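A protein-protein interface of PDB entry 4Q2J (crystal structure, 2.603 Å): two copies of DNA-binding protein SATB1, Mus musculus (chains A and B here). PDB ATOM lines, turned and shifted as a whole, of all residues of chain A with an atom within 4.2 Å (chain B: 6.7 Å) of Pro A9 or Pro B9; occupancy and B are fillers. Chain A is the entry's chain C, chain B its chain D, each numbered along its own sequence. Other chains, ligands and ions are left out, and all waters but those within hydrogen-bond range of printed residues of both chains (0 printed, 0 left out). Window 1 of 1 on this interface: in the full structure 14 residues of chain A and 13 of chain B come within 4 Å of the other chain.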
ATOM      1  N   LEU A   8     -12.977 -14.357 -36.500  1.00  0.00           N
ATOM      2  CA  LEU A   8     -12.416 -13.170 -35.881  1.00  0.00           C
ATOM      3  C   LEU A   8     -13.519 -12.219 -35.463  1.00  0.00           C
ATOM      4  O   LEU A   8     -14.420 -11.949 -36.249  1.00  0.00           O
ATOM      5  CB  LEU A   8     -11.542 -12.433 -36.897  1.00  0.00           C
ATOM      6  CG  LEU A   8     -10.043 -12.398 -36.666  1.00  0.00           C
ATOM      7  CD1 LEU A   8      -9.605 -13.580 -35.817  1.00  0.00           C
ATOM      8  CD2 LEU A   8      -9.359 -12.414 -38.009  1.00  0.00           C
ATOM      9  N   PRO A   9     -13.438 -11.678 -34.236  1.00  0.00           N
ATOM     10  CA  PRO A   9     -14.339 -10.608 -33.783  1.00  0.00           C
ATOM     11  C   PRO A   9     -14.007  -9.295 -34.484  1.00  0.00           C
ATOM     12  O   PRO A   9     -12.855  -8.866 -34.424  1.00  0.00           O
ATOM     13  CB  PRO A   9     -13.996 -10.454 -32.299  1.00  0.00           C
ATOM     14  CG  PRO A   9     -13.192 -11.637 -31.944  1.00  0.00           C
ATOM     15  CD  PRO A   9     -12.495 -12.076 -33.190  1.00  0.00           C
ATOM     16  N   VAL A  10     -14.974  -8.667 -35.143  1.00  0.00           N
ATOM     17  CA  VAL A  10     -14.739  -7.367 -35.737  1.00  0.00           C
ATOM     18  C   VAL A  10     -15.746  -6.387 -35.180  1.00  0.00           C
ATOM     19  O   VAL A  10     -16.936  -6.673 -35.175  1.00  0.00           O
ATOM     20  CB  VAL A  10     -14.904  -7.420 -37.253  1.00  0.00           C
ATOM     21  CG1 VAL A  10     -14.515  -6.072 -37.895  1.00  0.00           C
ATOM     22  CG2 VAL A  10     -14.092  -8.564 -37.829  1.00  0.00           C
ATOM     23  N   PHE A  32     -19.753  -5.779 -32.057  1.00  0.00           N
ATOM     24  CA  PHE A  32     -18.873  -6.817 -32.555  1.00  0.00           C
ATOM     25  C   PHE A  32     -19.606  -7.804 -33.432  1.00  0.00           C
ATOM     26  O   PHE A  32     -20.679  -8.267 -33.069  1.00  0.00           O
ATOM     27  CB  PHE A  32     -18.250  -7.578 -31.389  1.00  0.00           C
ATOM     28  CG  PHE A  32     -17.024  -6.928 -30.828  1.00  0.00           C
ATOM     29  CD1 PHE A  32     -15.861  -6.877 -31.567  1.00  0.00           C
ATOM     30  CD2 PHE A  32     -17.034  -6.385 -29.553  1.00  0.00           C
ATOM     31  CE1 PHE A  32     -14.734  -6.288 -31.050  1.00  0.00           C
ATOM     32  CE2 PHE A  32     -15.905  -5.793 -29.024  1.00  0.00           C
ATOM     33  CZ  PHE A  32     -14.756  -5.748 -29.768  1.00  0.00           C
ATOM     34  N   VAL A  33     -19.026  -8.133 -34.579  1.00  0.00           N
ATOM     35  CA  VAL A  33     -19.476  -9.294 -35.333  1.00  0.00           C
ATOM     36  C   VAL A  33     -18.341 -10.239 -35.719  1.00  0.00           C
ATOM     37  O   VAL A  33     -17.364  -9.835 -36.357  1.00  0.00           O
ATOM     38  CB  VAL A  33     -20.299  -8.918 -36.599  1.00  0.00           C
ATOM     39  CG1 VAL A  33     -19.986  -7.530 -37.036  1.00  0.00           C
ATOM     40  CG2 VAL A  33     -20.044  -9.919 -37.735  1.00  0.00           C
ATOM     41  N   LEU A  34     -18.500 -11.499 -35.321  1.00  0.00           N
ATOM     42  CA  LEU A  34     -17.660 -12.606 -35.765  1.00  0.00           C
ATOM     43  C   LEU A  34     -17.730 -12.791 -37.273  1.00  0.00           C
ATOM     44  O   LEU A  34     -18.811 -12.714 -37.863  1.00  0.00           O
ATOM     45  CB  LEU A  34     -18.144 -13.900 -35.112  1.00  0.00           C
ATOM     46  CG  LEU A  34     -18.218 -13.907 -33.592  1.00  0.00           C
ATOM     47  CD1 LEU A  34     -18.629 -15.291 -33.094  1.00  0.00           C
ATOM     48  CD2 LEU A  34     -16.854 -13.480 -33.004  1.00  0.00           C
ATOM     49  N   TYR A  95      -7.376  -7.038 -35.055  1.00  0.00           N
ATOM     50  CA  TYR A  95      -8.832  -6.983 -34.944  1.00  0.00           C
ATOM     51  C   TYR A  95      -9.285  -6.298 -33.656  1.00  0.00           C
ATOM     52  O   TYR A  95     -10.421  -5.844 -33.555  1.00  0.00           O
ATOM     53  CB  TYR A  95      -9.459  -8.380 -35.055  1.00  0.00           C
ATOM     54  CG  TYR A  95      -9.257  -9.284 -33.845  1.00  0.00           C
ATOM     55  CD1 TYR A  95      -9.978  -9.087 -32.665  1.00  0.00           C
ATOM     56  CD2 TYR A  95      -8.370 -10.344 -33.896  1.00  0.00           C
ATOM     57  CE1 TYR A  95      -9.799  -9.907 -31.572  1.00  0.00           C
ATOM     58  CE2 TYR A  95      -8.188 -11.158 -32.822  1.00  0.00           C
ATOM     59  CZ  TYR A  95      -8.901 -10.939 -31.665  1.00  0.00           C
ATOM     60  OH  TYR A  95      -8.697 -11.781 -30.597  1.00  0.00           O
ATOM     61  N   MET B   7     -20.911  -5.942 -25.904  1.00  0.00           N
ATOM     62  CA  MET B   7     -20.351  -7.290 -25.911  1.00  0.00           C
ATOM     63  C   MET B   7     -18.830  -7.289 -25.843  1.00  0.00           C
ATOM     64  O   MET B   7     -18.185  -6.270 -26.068  1.00  0.00           O
ATOM     65  CB  MET B   7     -20.797  -8.071 -27.155  1.00  0.00           C
ATOM     66  CG  MET B   7     -22.297  -8.085 -27.373  1.00  0.00           C
ATOM     67  SD  MET B   7     -23.163  -8.519 -25.860  1.00  0.00           S
ATOM     68  CE  MET B   7     -23.488 -10.259 -26.154  1.00  0.00           C
ATOM     69  N   LEU B   8     -18.278  -8.454 -25.541  1.00  0.00           N
ATOM     70  CA  LEU B   8     -16.854  -8.673 -25.577  1.00  0.00           C
ATOM     71  C   LEU B   8     -16.630 -10.084 -26.079  1.00  0.00           C
ATOM     72  O   LEU B   8     -17.230 -11.031 -25.560  1.00  0.00           O
ATOM     73  CB  LEU B   8     -16.282  -8.538 -24.180  1.00  0.00           C
ATOM     74  CG  LEU B   8     -14.908  -7.893 -24.143  1.00  0.00           C
ATOM     75  CD1 LEU B   8     -15.022  -6.469 -24.667  1.00  0.00           C
ATOM     76  CD2 LEU B   8     -14.348  -7.925 -22.719  1.00  0.00           C
ATOM     77  N   PRO B   9     -15.766 -10.240 -27.090  1.00  0.00           N
ATOM     78  CA  PRO B   9     -15.473 -11.574 -27.618  1.00  0.00           C
ATOM     79  C   PRO B   9     -14.617 -12.349 -26.617  1.00  0.00           C
ATOM     80  O   PRO B   9     -13.661 -11.793 -26.094  1.00  0.00           O
ATOM     81  CB  PRO B   9     -14.653 -11.282 -28.884  1.00  0.00           C
ATOM     82  CG  PRO B   9     -14.800  -9.820 -29.134  1.00  0.00           C
ATOM     83  CD  PRO B   9     -15.011  -9.199 -27.791  1.00  0.00           C
ATOM     84  N   VAL B  10     -14.962 -13.596 -26.330  1.00  0.00           N
ATOM     85  CA  VAL B  10     -14.109 -14.422 -25.497  1.00  0.00           C
ATOM     86  C   VAL B  10     -13.890 -15.759 -26.179  1.00  0.00           C
ATOM     87  O   VAL B  10     -14.845 -16.417 -26.570  1.00  0.00           O
ATOM     88  CB  VAL B  10     -14.700 -14.644 -24.098  1.00  0.00           C
ATOM     89  CG1 VAL B  10     -13.803 -15.567 -23.300  1.00  0.00           C
ATOM     90  CG2 VAL B  10     -14.891 -13.313 -23.371  1.00  0.00           C
ATOM     91  N   PHE B  11     -12.635 -16.154 -26.342  1.00  0.00           N
ATOM     92  CA  PHE B  11     -12.328 -17.455 -26.915  1.00  0.00           C
ATOM     93  C   PHE B  11     -12.505 -18.520 -25.846  1.00  0.00           C
ATOM     94  O   PHE B  11     -11.934 -18.409 -24.761  1.00  0.00           O
ATOM     95  CB  PHE B  11     -10.903 -17.478 -27.422  1.00  0.00           C
ATOM     96  CG  PHE B  11     -10.609 -18.597 -28.369  1.00  0.00           C
ATOM     97  CD1 PHE B  11     -10.792 -18.432 -29.730  1.00  0.00           C
ATOM     98  CD2 PHE B  11     -10.116 -19.794 -27.909  1.00  0.00           C
ATOM     99  CE1 PHE B  11     -10.501 -19.451 -30.609  1.00  0.00           C
ATOM    100  CE2 PHE B  11      -9.829 -20.820 -28.782  1.00  0.00           C
ATOM    101  CZ  PHE B  11     -10.016 -20.649 -30.129  1.00  0.00           C
ATOM    102  N   PHE B  32     -14.691 -17.977 -30.341  1.00  0.00           N
ATOM    103  CA  PHE B  32     -15.189 -16.786 -29.661  1.00  0.00           C
ATOM    104  C   PHE B  32     -16.675 -16.896 -29.369  1.00  0.00           C
ATOM    105  O   PHE B  32     -17.447 -17.330 -30.215  1.00  0.00           O
ATOM    106  CB  PHE B  32     -14.913 -15.527 -30.499  1.00  0.00           C
ATOM    107  CG  PHE B  32     -13.457 -15.217 -30.649  1.00  0.00           C
ATOM    108  CD1 PHE B  32     -12.782 -14.493 -29.665  1.00  0.00           C
ATOM    109  CD2 PHE B  32     -12.749 -15.673 -31.751  1.00  0.00           C
ATOM    110  CE1 PHE B  32     -11.442 -14.209 -29.789  1.00  0.00           C
ATOM    111  CE2 PHE B  32     -11.398 -15.401 -31.873  1.00  0.00           C
ATOM    112  CZ  PHE B  32     -10.750 -14.660 -30.892  1.00  0.00           C
ATOM    113  N   VAL B  33     -17.066 -16.516 -28.160  1.00  0.00           N
ATOM    114  CA  VAL B  33     -18.465 -16.270 -27.878  1.00  0.00           C
ATOM    115  C   VAL B  33     -18.590 -14.863 -27.321  1.00  0.00           C
ATOM    116  O   VAL B  33     -17.836 -14.466 -26.431  1.00  0.00           O
ATOM    117  CB  VAL B  33     -19.082 -17.289 -26.879  1.00  0.00           C
ATOM    118  CG1 VAL B  33     -18.240 -18.552 -26.787  1.00  0.00           C
ATOM    119  CG2 VAL B  33     -19.288 -16.657 -25.519  1.00  0.00           C
ATOM    120  N   LEU B  34     -19.535 -14.108 -27.865  1.00  0.00           N
ATOM    121  CA  LEU B  34     -19.829 -12.775 -27.364  1.00  0.00           C
ATOM    122  C   LEU B  34     -20.543 -12.846 -26.019  1.00  0.00           C
ATOM    123  O   LEU B  34     -21.542 -13.526 -25.878  1.00  0.00           O
ATOM    124  CB  LEU B  34     -20.678 -12.012 -28.376  1.00  0.00           C
ATOM    125  CG  LEU B  34     -19.992 -11.745 -29.713  1.00  0.00           C
ATOM    126  CD1 LEU B  34     -20.972 -11.088 -30.714  1.00  0.00           C
ATOM    127  CD2 LEU B  34     -18.725 -10.888 -29.506  1.00  0.00           C
ATOM    128  N   VAL B  35     -20.024 -12.151 -25.026  1.00  0.00           N
ATOM    129  CA  VAL B  35     -20.686 -12.096 -23.740  1.00  0.00           C
ATOM    130  C   VAL B  35     -20.935 -10.646 -23.376  1.00  0.00           C
ATOM    131  O   VAL B  35     -20.441  -9.738 -24.027  1.00  0.00           O
ATOM    132  CB  VAL B  35     -19.854 -12.766 -22.618  1.00  0.00           C
ATOM    133  CG1 VAL B  35     -19.176 -14.027 -23.134  1.00  0.00           C
ATOM    134  CG2 VAL B  35     -18.833 -11.796 -22.093  1.00  0.00           C
ATOM    135  N   LEU B  91     -11.326  -8.096 -18.593  1.00  0.00           N
ATOM    136  CA  LEU B  91     -10.895  -8.650 -19.874  1.00  0.00           C
ATOM    137  C   LEU B  91     -10.979  -7.633 -20.990  1.00  0.00           C
ATOM    138  O   LEU B  91     -10.624  -7.922 -22.139  1.00  0.00           O
ATOM    139  CB  LEU B  91     -11.745  -9.868 -20.235  1.00  0.00           C
ATOM    140  CG  LEU B  91     -11.947 -10.997 -19.219  1.00  0.00           C
ATOM    141  CD1 LEU B  91     -12.902 -11.982 -19.809  1.00  0.00           C
ATOM    142  CD2 LEU B  91     -10.624 -11.688 -18.893  1.00  0.00           C
ATOM    143  N   TYR B  95      -8.863  -9.438 -23.868  1.00  0.00           N
ATOM    144  CA  TYR B  95      -9.727 -10.429 -24.508  1.00  0.00           C
ATOM    145  C   TYR B  95      -9.093 -11.055 -25.750  1.00  0.00           C
ATOM    146  O   TYR B  95      -9.447 -12.160 -26.136  1.00  0.00           O
ATOM    147  CB  TYR B  95     -11.127  -9.864 -24.808  1.00  0.00           C
ATOM    148  CG  TYR B  95     -11.227  -8.927 -25.993  1.00  0.00           C
ATOM    149  CD1 TYR B  95     -11.143  -9.404 -27.295  1.00  0.00           C
ATOM    150  CD2 TYR B  95     -11.442  -7.563 -25.802  1.00  0.00           C
ATOM    151  CE1 TYR B  95     -11.232  -8.532 -28.384  1.00  0.00           C
ATOM    152  CE2 TYR B  95     -11.541  -6.690 -26.868  1.00  0.00           C
ATOM    153  CZ  TYR B  95     -11.437  -7.173 -28.162  1.00  0.00           C
ATOM    154  OH  TYR B  95     -11.541  -6.287 -29.238  1.00  0.00           O
ATOM    155  N   HIS B  96      -8.146 -10.358 -26.365  1.00  0.00           N
ATOM    156  CA  HIS B  96      -7.494 -10.848 -27.585  1.00  0.00           C
ATOM    157  C   HIS B  96      -6.366 -11.838 -27.304  1.00  0.00           C
ATOM    158  O   HIS B  96      -5.844 -12.460 -28.232  1.00  0.00           O
ATOM    159  CB  HIS B  96      -6.953  -9.676 -28.407  1.00  0.00           C
ATOM    160  CG  HIS B  96      -6.207  -8.670 -27.592  1.00  0.00           C
ATOM    161  ND1 HIS B  96      -6.839  -7.786 -26.741  1.00  0.00           N
ATOM    162  CD2 HIS B  96      -4.879  -8.421 -27.478  1.00  0.00           C
ATOM    163  CE1 HIS B  96      -5.930  -7.037 -26.139  1.00  0.00           C
ATOM    164  NE2 HIS B  96      -4.735  -7.398 -26.571  1.00  0.00           N
ATOM    165  N   VAL B  98      -6.402 -13.820 -24.106  1.00  0.00           N
ATOM    166  CA  VAL B  98      -6.832 -14.857 -23.181  1.00  0.00           C
ATOM    167  C   VAL B  98      -7.719 -15.928 -23.842  1.00  0.00           C
ATOM    168  O   VAL B  98      -8.417 -15.679 -24.837  1.00  0.00           O
ATOM    169  CB  VAL B  98      -7.459 -14.280 -21.889  1.00  0.00           C
ATOM    170  CG1 VAL B  98      -6.420 -13.421 -21.132  1.00  0.00           C
ATOM    171  CG2 VAL B  98      -8.686 -13.477 -22.200  1.00  0.00           C
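Pro B9 touches its own counterpart, Pro A9.
Pro A9 touches Phe B32, and with the chains exchanged Phe A32 touches Pro B9.
Phe A32 touches Leu B34, and with the chains exchanged Leu A34 touches Phe B32.
Tyr A95 touches its own counterpart, Tyr B95.
Of the 10 pairs that touch across the chains among the printed residues, 8 have their exchanged pair printed and touching as well.
Pro B9 touches Pro A9.
CG of Pro A9 touches CD1 of Phe B32 (3.7 Å).
CD2 of Phe A32 touches O of Met B7, 3.7 Å away.
Pro B9 touches Phe A32.
Leu B34 touches Phe A32.
Phe A32 touches Tyr B95.
Phe B32 touches Leu A34 (O to CD1, 3.7 Å).
Tyr A95 touches Phe B32.
Tyr B95 touches Tyr A95.
Tyr A95 touches His B96.
Of the 13 printed residues of chain B, 6 touch a printed residue of chain A.
Printed residues of chain B that touch a printed residue of chain A: Met B7, Pro B9, Phe B32, Leu B34, Tyr B95 and His B96.
Hydrophobic or aromatic side chains of chain B that line the printed part of chain A: Pro B9, Phe B32, Leu B34, Tyr B95 and His B96.
Printed residues of chain A that touch a printed residue of chain B: Pro A9, Phe A32, Leu A34 and Tyr A95.
Hydrophobic or aromatic side chains of chain A that line the printed part of chain B: Pro A9, Phe A32, Leu A34 and Tyr A95.
Among the printed residues, 10 pairs touch across the chains.
Pro A9 touches two residues of chain B.
Printed residues of chain B within 4 Å of Phe A32: Met B7 (3.7 Å), Pro B9 (3.7 Å), Leu B34 (3.7 Å) and Tyr B95 (3.3 Å).
Printed residues of chain A within 4 Å of Met B7: Phe A32 (3.7 Å).
Of the printed residues of chain A, Pro B9 touches Pro A9 and Phe A32.
Printed residues of chain A within 4 Å of Tyr B95: Phe A32 (3.3 Å) and Tyr A95 (3.8 Å).
Printed residues of chain A within 4 Å of His B96: Tyr A95.
Val B98 touches none of the printed residues of chain A.
The nearest residue of chain B that does not touch Pro A9 is Tyr B95 (5.1 Å).
The nearest printed residue of chain A that does not touch Tyr B95 is Pro A9 (5.1 Å).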
